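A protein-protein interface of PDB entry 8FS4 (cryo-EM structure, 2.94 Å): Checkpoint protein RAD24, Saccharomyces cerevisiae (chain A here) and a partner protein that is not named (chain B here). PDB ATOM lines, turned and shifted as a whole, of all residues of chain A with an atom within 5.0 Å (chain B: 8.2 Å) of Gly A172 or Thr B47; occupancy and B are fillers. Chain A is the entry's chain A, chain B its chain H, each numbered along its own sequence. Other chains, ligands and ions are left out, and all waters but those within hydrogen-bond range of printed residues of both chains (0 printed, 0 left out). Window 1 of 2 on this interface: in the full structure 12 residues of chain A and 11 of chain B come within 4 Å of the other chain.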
ATOM      1  N   THR A 149      14.324  16.386  33.376  1.00  0.00           N
ATOM      2  CA  THR A 149      14.773  17.455  32.482  1.00  0.00           C
ATOM      3  C   THR A 149      16.150  17.122  31.907  1.00  0.00           C
ATOM      4  O   THR A 149      17.159  17.709  32.304  1.00  0.00           O
ATOM      5  CB  THR A 149      14.764  18.802  33.232  1.00  0.00           C
ATOM      6  OG1 THR A 149      13.428  19.314  33.241  1.00  0.00           O
ATOM      7  CG2 THR A 149      15.648  19.881  32.563  1.00  0.00           C
ATOM      8  N   SER A 167      24.340  26.378  26.171  1.00  0.00           N
ATOM      9  CA  SER A 167      24.208  27.623  26.924  1.00  0.00           C
ATOM     10  C   SER A 167      22.750  28.053  27.009  1.00  0.00           C
ATOM     11  O   SER A 167      22.255  28.402  28.087  1.00  0.00           O
ATOM     12  CB  SER A 167      25.054  28.717  26.275  1.00  0.00           C
ATOM     13  OG  SER A 167      25.443  29.691  27.225  1.00  0.00           O
ATOM     14  N   GLU A 168      22.042  28.033  25.879  1.00  0.00           N
ATOM     15  CA  GLU A 168      20.625  28.373  25.897  1.00  0.00           C
ATOM     16  C   GLU A 168      19.846  27.387  26.754  1.00  0.00           C
ATOM     17  O   GLU A 168      18.925  27.776  27.484  1.00  0.00           O
ATOM     18  CB  GLU A 168      20.072  28.399  24.472  1.00  0.00           C
ATOM     19  CG  GLU A 168      20.815  29.335  23.533  1.00  0.00           C
ATOM     20  CD  GLU A 168      20.845  30.765  24.032  1.00  0.00           C
ATOM     21  OE1 GLU A 168      19.965  31.135  24.837  1.00  0.00           O
ATOM     22  OE2 GLU A 168      21.750  31.519  23.619  1.00  0.00           O
ATOM     23  N   PHE A 169      20.197  26.104  26.677  1.00  0.00           N
ATOM     24  CA  PHE A 169      19.546  25.105  27.516  1.00  0.00           C
ATOM     25  C   PHE A 169      19.773  25.402  28.992  1.00  0.00           C
ATOM     26  O   PHE A 169      18.827  25.413  29.789  1.00  0.00           O
ATOM     27  CB  PHE A 169      20.066  23.714  27.163  1.00  0.00           C
ATOM     28  CG  PHE A 169      19.962  22.729  28.288  1.00  0.00           C
ATOM     29  CD1 PHE A 169      18.766  22.087  28.552  1.00  0.00           C
ATOM     30  CD2 PHE A 169      21.062  22.438  29.077  1.00  0.00           C
ATOM     31  CE1 PHE A 169      18.666  21.179  29.583  1.00  0.00           C
ATOM     32  CE2 PHE A 169      20.966  21.528  30.109  1.00  0.00           C
ATOM     33  CZ  PHE A 169      19.765  20.899  30.361  1.00  0.00           C
ATOM     34  N   LEU A 170      21.028  25.645  29.379  1.00  0.00           N
ATOM     35  CA  LEU A 170      21.315  25.938  30.779  1.00  0.00           C
ATOM     36  C   LEU A 170      20.894  27.353  31.152  1.00  0.00           C
ATOM     37  O   LEU A 170      20.637  27.629  32.329  1.00  0.00           O
ATOM     38  CB  LEU A 170      22.800  25.728  31.075  1.00  0.00           C
ATOM     39  CG  LEU A 170      23.261  24.294  31.369  1.00  0.00           C
ATOM     40  CD1 LEU A 170      24.694  24.310  31.851  1.00  0.00           C
ATOM     41  CD2 LEU A 170      22.379  23.584  32.392  1.00  0.00           C
ATOM     42  N   LYS A 171      20.821  28.259  30.176  1.00  0.00           N
ATOM     43  CA  LYS A 171      20.264  29.578  30.453  1.00  0.00           C
ATOM     44  C   LYS A 171      18.806  29.474  30.877  1.00  0.00           C
ATOM     45  O   LYS A 171      18.307  30.338  31.607  1.00  0.00           O
ATOM     46  CB  LYS A 171      20.403  30.475  29.226  1.00  0.00           C
ATOM     47  CG  LYS A 171      21.762  31.144  29.101  1.00  0.00           C
ATOM     48  CD  LYS A 171      21.965  31.720  27.708  1.00  0.00           C
ATOM     49  CE  LYS A 171      23.323  32.390  27.562  1.00  0.00           C
ATOM     50  NZ  LYS A 171      23.689  33.210  28.749  1.00  0.00           N
ATOM     51  N   GLY A 172      18.110  28.430  30.427  1.00  0.00           N
ATOM     52  CA  GLY A 172      16.772  28.123  30.888  1.00  0.00           C
ATOM     53  C   GLY A 172      16.681  26.944  31.829  1.00  0.00           C
ATOM     54  O   GLY A 172      15.564  26.503  32.135  1.00  0.00           O
ATOM     55  N   ALA A 173      17.806  26.406  32.298  1.00  0.00           N
ATOM     56  CA  ALA A 173      17.818  25.308  33.255  1.00  0.00           C
ATOM     57  C   ALA A 173      17.993  25.790  34.685  1.00  0.00           C
ATOM     58  O   ALA A 173      18.153  24.967  35.592  1.00  0.00           O
ATOM     59  CB  ALA A 173      18.925  24.315  32.910  1.00  0.00           C
ATOM     60  N   ARG A 174      17.979  27.106  34.906  1.00  0.00           N
ATOM     61  CA  ARG A 174      18.101  27.680  36.236  1.00  0.00           C
ATOM     62  C   ARG A 174      16.770  28.135  36.806  1.00  0.00           C
ATOM     63  O   ARG A 174      16.648  28.258  38.029  1.00  0.00           O
ATOM     64  CB  ARG A 174      19.064  28.877  36.216  1.00  0.00           C
ATOM     65  CG  ARG A 174      20.316  28.662  35.377  1.00  0.00           C
ATOM     66  CD  ARG A 174      20.711  29.919  34.626  1.00  0.00           C
ATOM     67  NE  ARG A 174      22.114  29.893  34.233  1.00  0.00           N
ATOM     68  CZ  ARG A 174      23.133  29.953  35.079  1.00  0.00           C
ATOM     69  NH1 ARG A 174      22.942  30.061  36.385  1.00  0.00           N
ATOM     70  NH2 ARG A 174      24.374  29.901  34.606  1.00  0.00           N
ATOM     71  N   TYR A 175      15.775  28.381  35.953  1.00  0.00           N
ATOM     72  CA  TYR A 175      14.443  28.746  36.405  1.00  0.00           C
ATOM     73  C   TYR A 175      13.695  27.576  37.024  1.00  0.00           C
ATOM     74  O   TYR A 175      12.597  27.778  37.554  1.00  0.00           O
ATOM     75  CB  TYR A 175      13.634  29.312  35.239  1.00  0.00           C
ATOM     76  CG  TYR A 175      14.096  30.677  34.792  1.00  0.00           C
ATOM     77  CD1 TYR A 175      15.173  30.817  33.928  1.00  0.00           C
ATOM     78  CD2 TYR A 175      13.456  31.827  35.231  1.00  0.00           C
ATOM     79  CE1 TYR A 175      15.601  32.063  33.516  1.00  0.00           C
ATOM     80  CE2 TYR A 175      13.875  33.078  34.823  1.00  0.00           C
ATOM     81  CZ  TYR A 175      14.949  33.190  33.967  1.00  0.00           C
ATOM     82  OH  TYR A 175      15.372  34.434  33.559  1.00  0.00           O
ATOM     83  N   LEU A 176      14.254  26.366  36.977  1.00  0.00           N
ATOM     84  CA  LEU A 176      13.594  25.215  37.579  1.00  0.00           C
ATOM     85  C   LEU A 176      13.783  25.245  39.093  1.00  0.00           C
ATOM     86  O   LEU A 176      14.242  24.272  39.698  1.00  0.00           O
ATOM     87  CB  LEU A 176      14.133  23.915  36.984  1.00  0.00           C
ATOM     88  CG  LEU A 176      14.005  23.791  35.462  1.00  0.00           C
ATOM     89  CD1 LEU A 176      14.546  22.451  34.994  1.00  0.00           C
ATOM     90  CD2 LEU A 176      12.560  23.971  35.008  1.00  0.00           C
ATOM     91  N   GLN B  27      11.662  25.735  18.578  1.00  0.00           N
ATOM     92  CA  GLN B  27      11.877  24.295  18.644  1.00  0.00           C
ATOM     93  C   GLN B  27      12.196  23.773  17.251  1.00  0.00           C
ATOM     94  O   GLN B  27      11.729  24.317  16.247  1.00  0.00           O
ATOM     95  CB  GLN B  27      10.651  23.565  19.216  1.00  0.00           C
ATOM     96  CG  GLN B  27      10.879  22.088  19.521  1.00  0.00           C
ATOM     97  CD  GLN B  27      11.685  21.867  20.785  1.00  0.00           C
ATOM     98  OE1 GLN B  27      12.901  22.058  20.802  1.00  0.00           O
ATOM     99  NE2 GLN B  27      11.011  21.457  21.853  1.00  0.00           N
ATOM    100  N   MET B  44       7.578  24.697  21.694  1.00  0.00           N
ATOM    101  CA  MET B  44       7.957  24.454  23.078  1.00  0.00           C
ATOM    102  C   MET B  44       9.456  24.684  23.230  1.00  0.00           C
ATOM    103  O   MET B  44      10.166  24.957  22.258  1.00  0.00           O
ATOM    104  CB  MET B  44       7.582  23.032  23.516  1.00  0.00           C
ATOM    105  CG  MET B  44       6.088  22.774  23.579  1.00  0.00           C
ATOM    106  SD  MET B  44       5.235  23.863  24.732  1.00  0.00           S
ATOM    107  CE  MET B  44       3.570  23.765  24.087  1.00  0.00           C
ATOM    108  N   ASN B  45       9.938  24.563  24.464  1.00  0.00           N
ATOM    109  CA  ASN B  45      11.339  24.776  24.787  1.00  0.00           C
ATOM    110  C   ASN B  45      11.925  23.526  25.427  1.00  0.00           C
ATOM    111  O   ASN B  45      11.203  22.647  25.908  1.00  0.00           O
ATOM    112  CB  ASN B  45      11.517  25.971  25.732  1.00  0.00           C
ATOM    113  CG  ASN B  45      12.836  26.686  25.522  1.00  0.00           C
ATOM    114  OD1 ASN B  45      13.766  26.140  24.928  1.00  0.00           O
ATOM    115  ND2 ASN B  45      12.925  27.916  26.011  1.00  0.00           N
ATOM    116  N   GLU B  46      13.258  23.455  25.426  1.00  0.00           N
ATOM    117  CA  GLU B  46      13.934  22.300  26.006  1.00  0.00           C
ATOM    118  C   GLU B  46      13.682  22.205  27.503  1.00  0.00           C
ATOM    119  O   GLU B  46      13.391  21.121  28.025  1.00  0.00           O
ATOM    120  CB  GLU B  46      15.434  22.375  25.722  1.00  0.00           C
ATOM    121  CG  GLU B  46      16.239  21.289  26.411  1.00  0.00           C
ATOM    122  CD  GLU B  46      15.692  19.906  26.132  1.00  0.00           C
ATOM    123  OE1 GLU B  46      15.120  19.703  25.040  1.00  0.00           O
ATOM    124  OE2 GLU B  46      15.833  19.022  27.002  1.00  0.00           O
ATOM    125  N   THR B  47      13.789  23.326  28.215  1.00  0.00           N
ATOM    126  CA  THR B  47      13.555  23.371  29.651  1.00  0.00           C
ATOM    127  C   THR B  47      12.114  23.736  29.987  1.00  0.00           C
ATOM    128  O   THR B  47      11.824  24.105  31.130  1.00  0.00           O
ATOM    129  CB  THR B  47      14.523  24.356  30.310  1.00  0.00           C
ATOM    130  OG1 THR B  47      14.489  25.607  29.611  1.00  0.00           O
ATOM    131  CG2 THR B  47      15.942  23.805  30.286  1.00  0.00           C
ATOM    132  N   ASP B  48      11.209  23.637  29.015  1.00  0.00           N
ATOM    133  CA  ASP B  48       9.789  23.927  29.205  1.00  0.00           C
ATOM    134  C   ASP B  48       9.600  25.284  29.888  1.00  0.00           C
ATOM    135  O   ASP B  48       9.074  25.399  30.996  1.00  0.00           O
ATOM    136  CB  ASP B  48       9.117  22.807  30.003  1.00  0.00           C
ATOM    137  CG  ASP B  48       9.155  21.476  29.281  1.00  0.00           C
ATOM    138  OD1 ASP B  48       9.923  21.352  28.305  1.00  0.00           O
ATOM    139  OD2 ASP B  48       8.416  20.555  29.688  1.00  0.00           O
ATOM    140  N   THR B  49      10.051  26.317  29.183  1.00  0.00           N
ATOM    141  CA  THR B  49      10.003  27.686  29.680  1.00  0.00           C
ATOM    142  C   THR B  49       9.101  28.595  28.862  1.00  0.00           C
ATOM    143  O   THR B  49       8.320  29.356  29.437  1.00  0.00           O
ATOM    144  CB  THR B  49      11.421  28.279  29.714  1.00  0.00           C
ATOM    145  OG1 THR B  49      11.965  28.309  28.390  1.00  0.00           O
ATOM    146  CG2 THR B  49      12.323  27.451  30.619  1.00  0.00           C
ATOM    147  N   THR B  50       9.180  28.536  27.535  1.00  0.00           N
ATOM    148  CA  THR B  50       8.419  29.414  26.661  1.00  0.00           C
ATOM    149  C   THR B  50       7.356  28.626  25.908  1.00  0.00           C
ATOM    150  O   THR B  50       7.512  27.431  25.641  1.00  0.00           O
ATOM    151  CB  THR B  50       9.334  30.123  25.657  1.00  0.00           C
ATOM    152  OG1 THR B  50       9.745  29.198  24.644  1.00  0.00           O
ATOM    153  CG2 THR B  50      10.559  30.685  26.358  1.00  0.00           C
ATOM    154  N   LYS B 325      13.452  36.166  29.479  1.00  0.00           N
ATOM    155  CA  LYS B 325      14.469  36.002  28.444  1.00  0.00           C
ATOM    156  C   LYS B 325      14.309  37.065  27.353  1.00  0.00           C
ATOM    157  O   LYS B 325      13.489  37.981  27.447  1.00  0.00           O
ATOM    158  CB  LYS B 325      14.391  34.590  27.877  1.00  0.00           C
ATOM    159  CG  LYS B 325      14.800  33.513  28.874  1.00  0.00           C
ATOM    160  CD  LYS B 325      15.541  32.371  28.203  1.00  0.00           C
ATOM    161  CE  LYS B 325      16.829  32.852  27.553  1.00  0.00           C
ATOM    162  NZ  LYS B 325      17.847  31.777  27.459  1.00  0.00           N
ATOM    163  N   LYS B 327      15.672  36.064  23.655  1.00  0.00           N
ATOM    164  CA  LYS B 327      15.831  35.499  22.320  1.00  0.00           C
ATOM    165  C   LYS B 327      14.494  35.242  21.640  1.00  0.00           C
ATOM    166  O   LYS B 327      14.441  35.187  20.406  1.00  0.00           O
ATOM    167  CB  LYS B 327      16.639  34.202  22.386  1.00  0.00           C
ATOM    168  CG  LYS B 327      15.865  32.997  22.901  1.00  0.00           C
ATOM    169  CD  LYS B 327      16.729  32.128  23.801  1.00  0.00           C
ATOM    170  CE  LYS B 327      16.472  30.648  23.587  1.00  0.00           C
ATOM    171  NZ  LYS B 327      16.776  29.865  24.817  1.00  0.00           N
ATOM    172  N   VAL B 376       8.190  32.027  31.259  1.00  0.00           N
ATOM    173  CA  VAL B 376       8.347  31.949  32.706  1.00  0.00           C
ATOM    174  C   VAL B 376       9.264  33.068  33.178  1.00  0.00           C
ATOM    175  O   VAL B 376      10.096  33.586  32.423  1.00  0.00           O
ATOM    176  CB  VAL B 376       8.886  30.564  33.122  1.00  0.00           C
ATOM    177  CG1 VAL B 376      10.197  30.259  32.413  1.00  0.00           C
ATOM    178  CG2 VAL B 376       9.058  30.483  34.633  1.00  0.00           C
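The side-chain carboxylate of Glu A168 is in salt-bridge range of the side-chain amino group of Lys B327, 3.4 Å away.
The side-chain hydroxyl (OG1) of Thr B47 sits at hydrogen-bond distance from the backbone carbonyl oxygen (O) of Gly A172, at 2.9 Å.
NZ of Lys B325 is in salt-bridge range of OE1 of Glu A168.
Among the printed residues, pairs that only touch across the chains: Phe A169 with Thr B47 (3.3 Å), Lys A171 with Lys B325 (3.4 Å), Phe A169 with Glu B46 (3.4 Å), Gly A172 with Thr B49 (3.7 Å), Ala A173 with Thr B47 (3.8 Å) and Leu A176 with Thr B47 (3.9 Å).
Ser A167 touches none of the printed residues of chain B.
Printed residues of chain B within 4 Å of Glu A168: Lys B325 and Lys B327.
Printed residues of chain B within 4 Å of Gly A172: Thr B47 and Thr B49.
Of chain A, only Phe A169, Gly A172, Ala A173 and Leu A176 come within 4 Å of Thr B47.
Thr B50 touches none of the printed residues of chain A.
Of the printed residues of chain A, Lys B327 touches Glu A168.
The nearest residue of chain B that does not touch Gly A172 is Lys B325 (4.5 Å).
The nearest residue of chain A that does not touch Thr B47 is Thr A149 (4.5 Å).
Of the 11 printed residues of chain B, 5 touch a printed residue of chain A.
Printed residues of chain B that touch a printed residue of chain A: Glu B46, Thr B47, Thr B49, Lys B325 and Lys B327.
Printed residues of chain A that touch a printed residue of chain B: Glu A168, Phe A169, Lys A171, Gly A172, Ala A173 and Leu A176.
Among the printed residues, Asp or Glu carboxylates within 4 Å of a Lys or Arg side-chain nitrogen of the other chain: Glu A168 with Lys B325 and Glu A168 with Lys B327.
N of Val B376 is in hydrogen-bond range of O of Thr B49, at 3.2 Å.
The side-chain hydroxyl (OG1) of Thr B49 lies within hydrogen-bond range of the side-chain amide nitrogen (ND2) of Asn B45 (2.6 Å).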
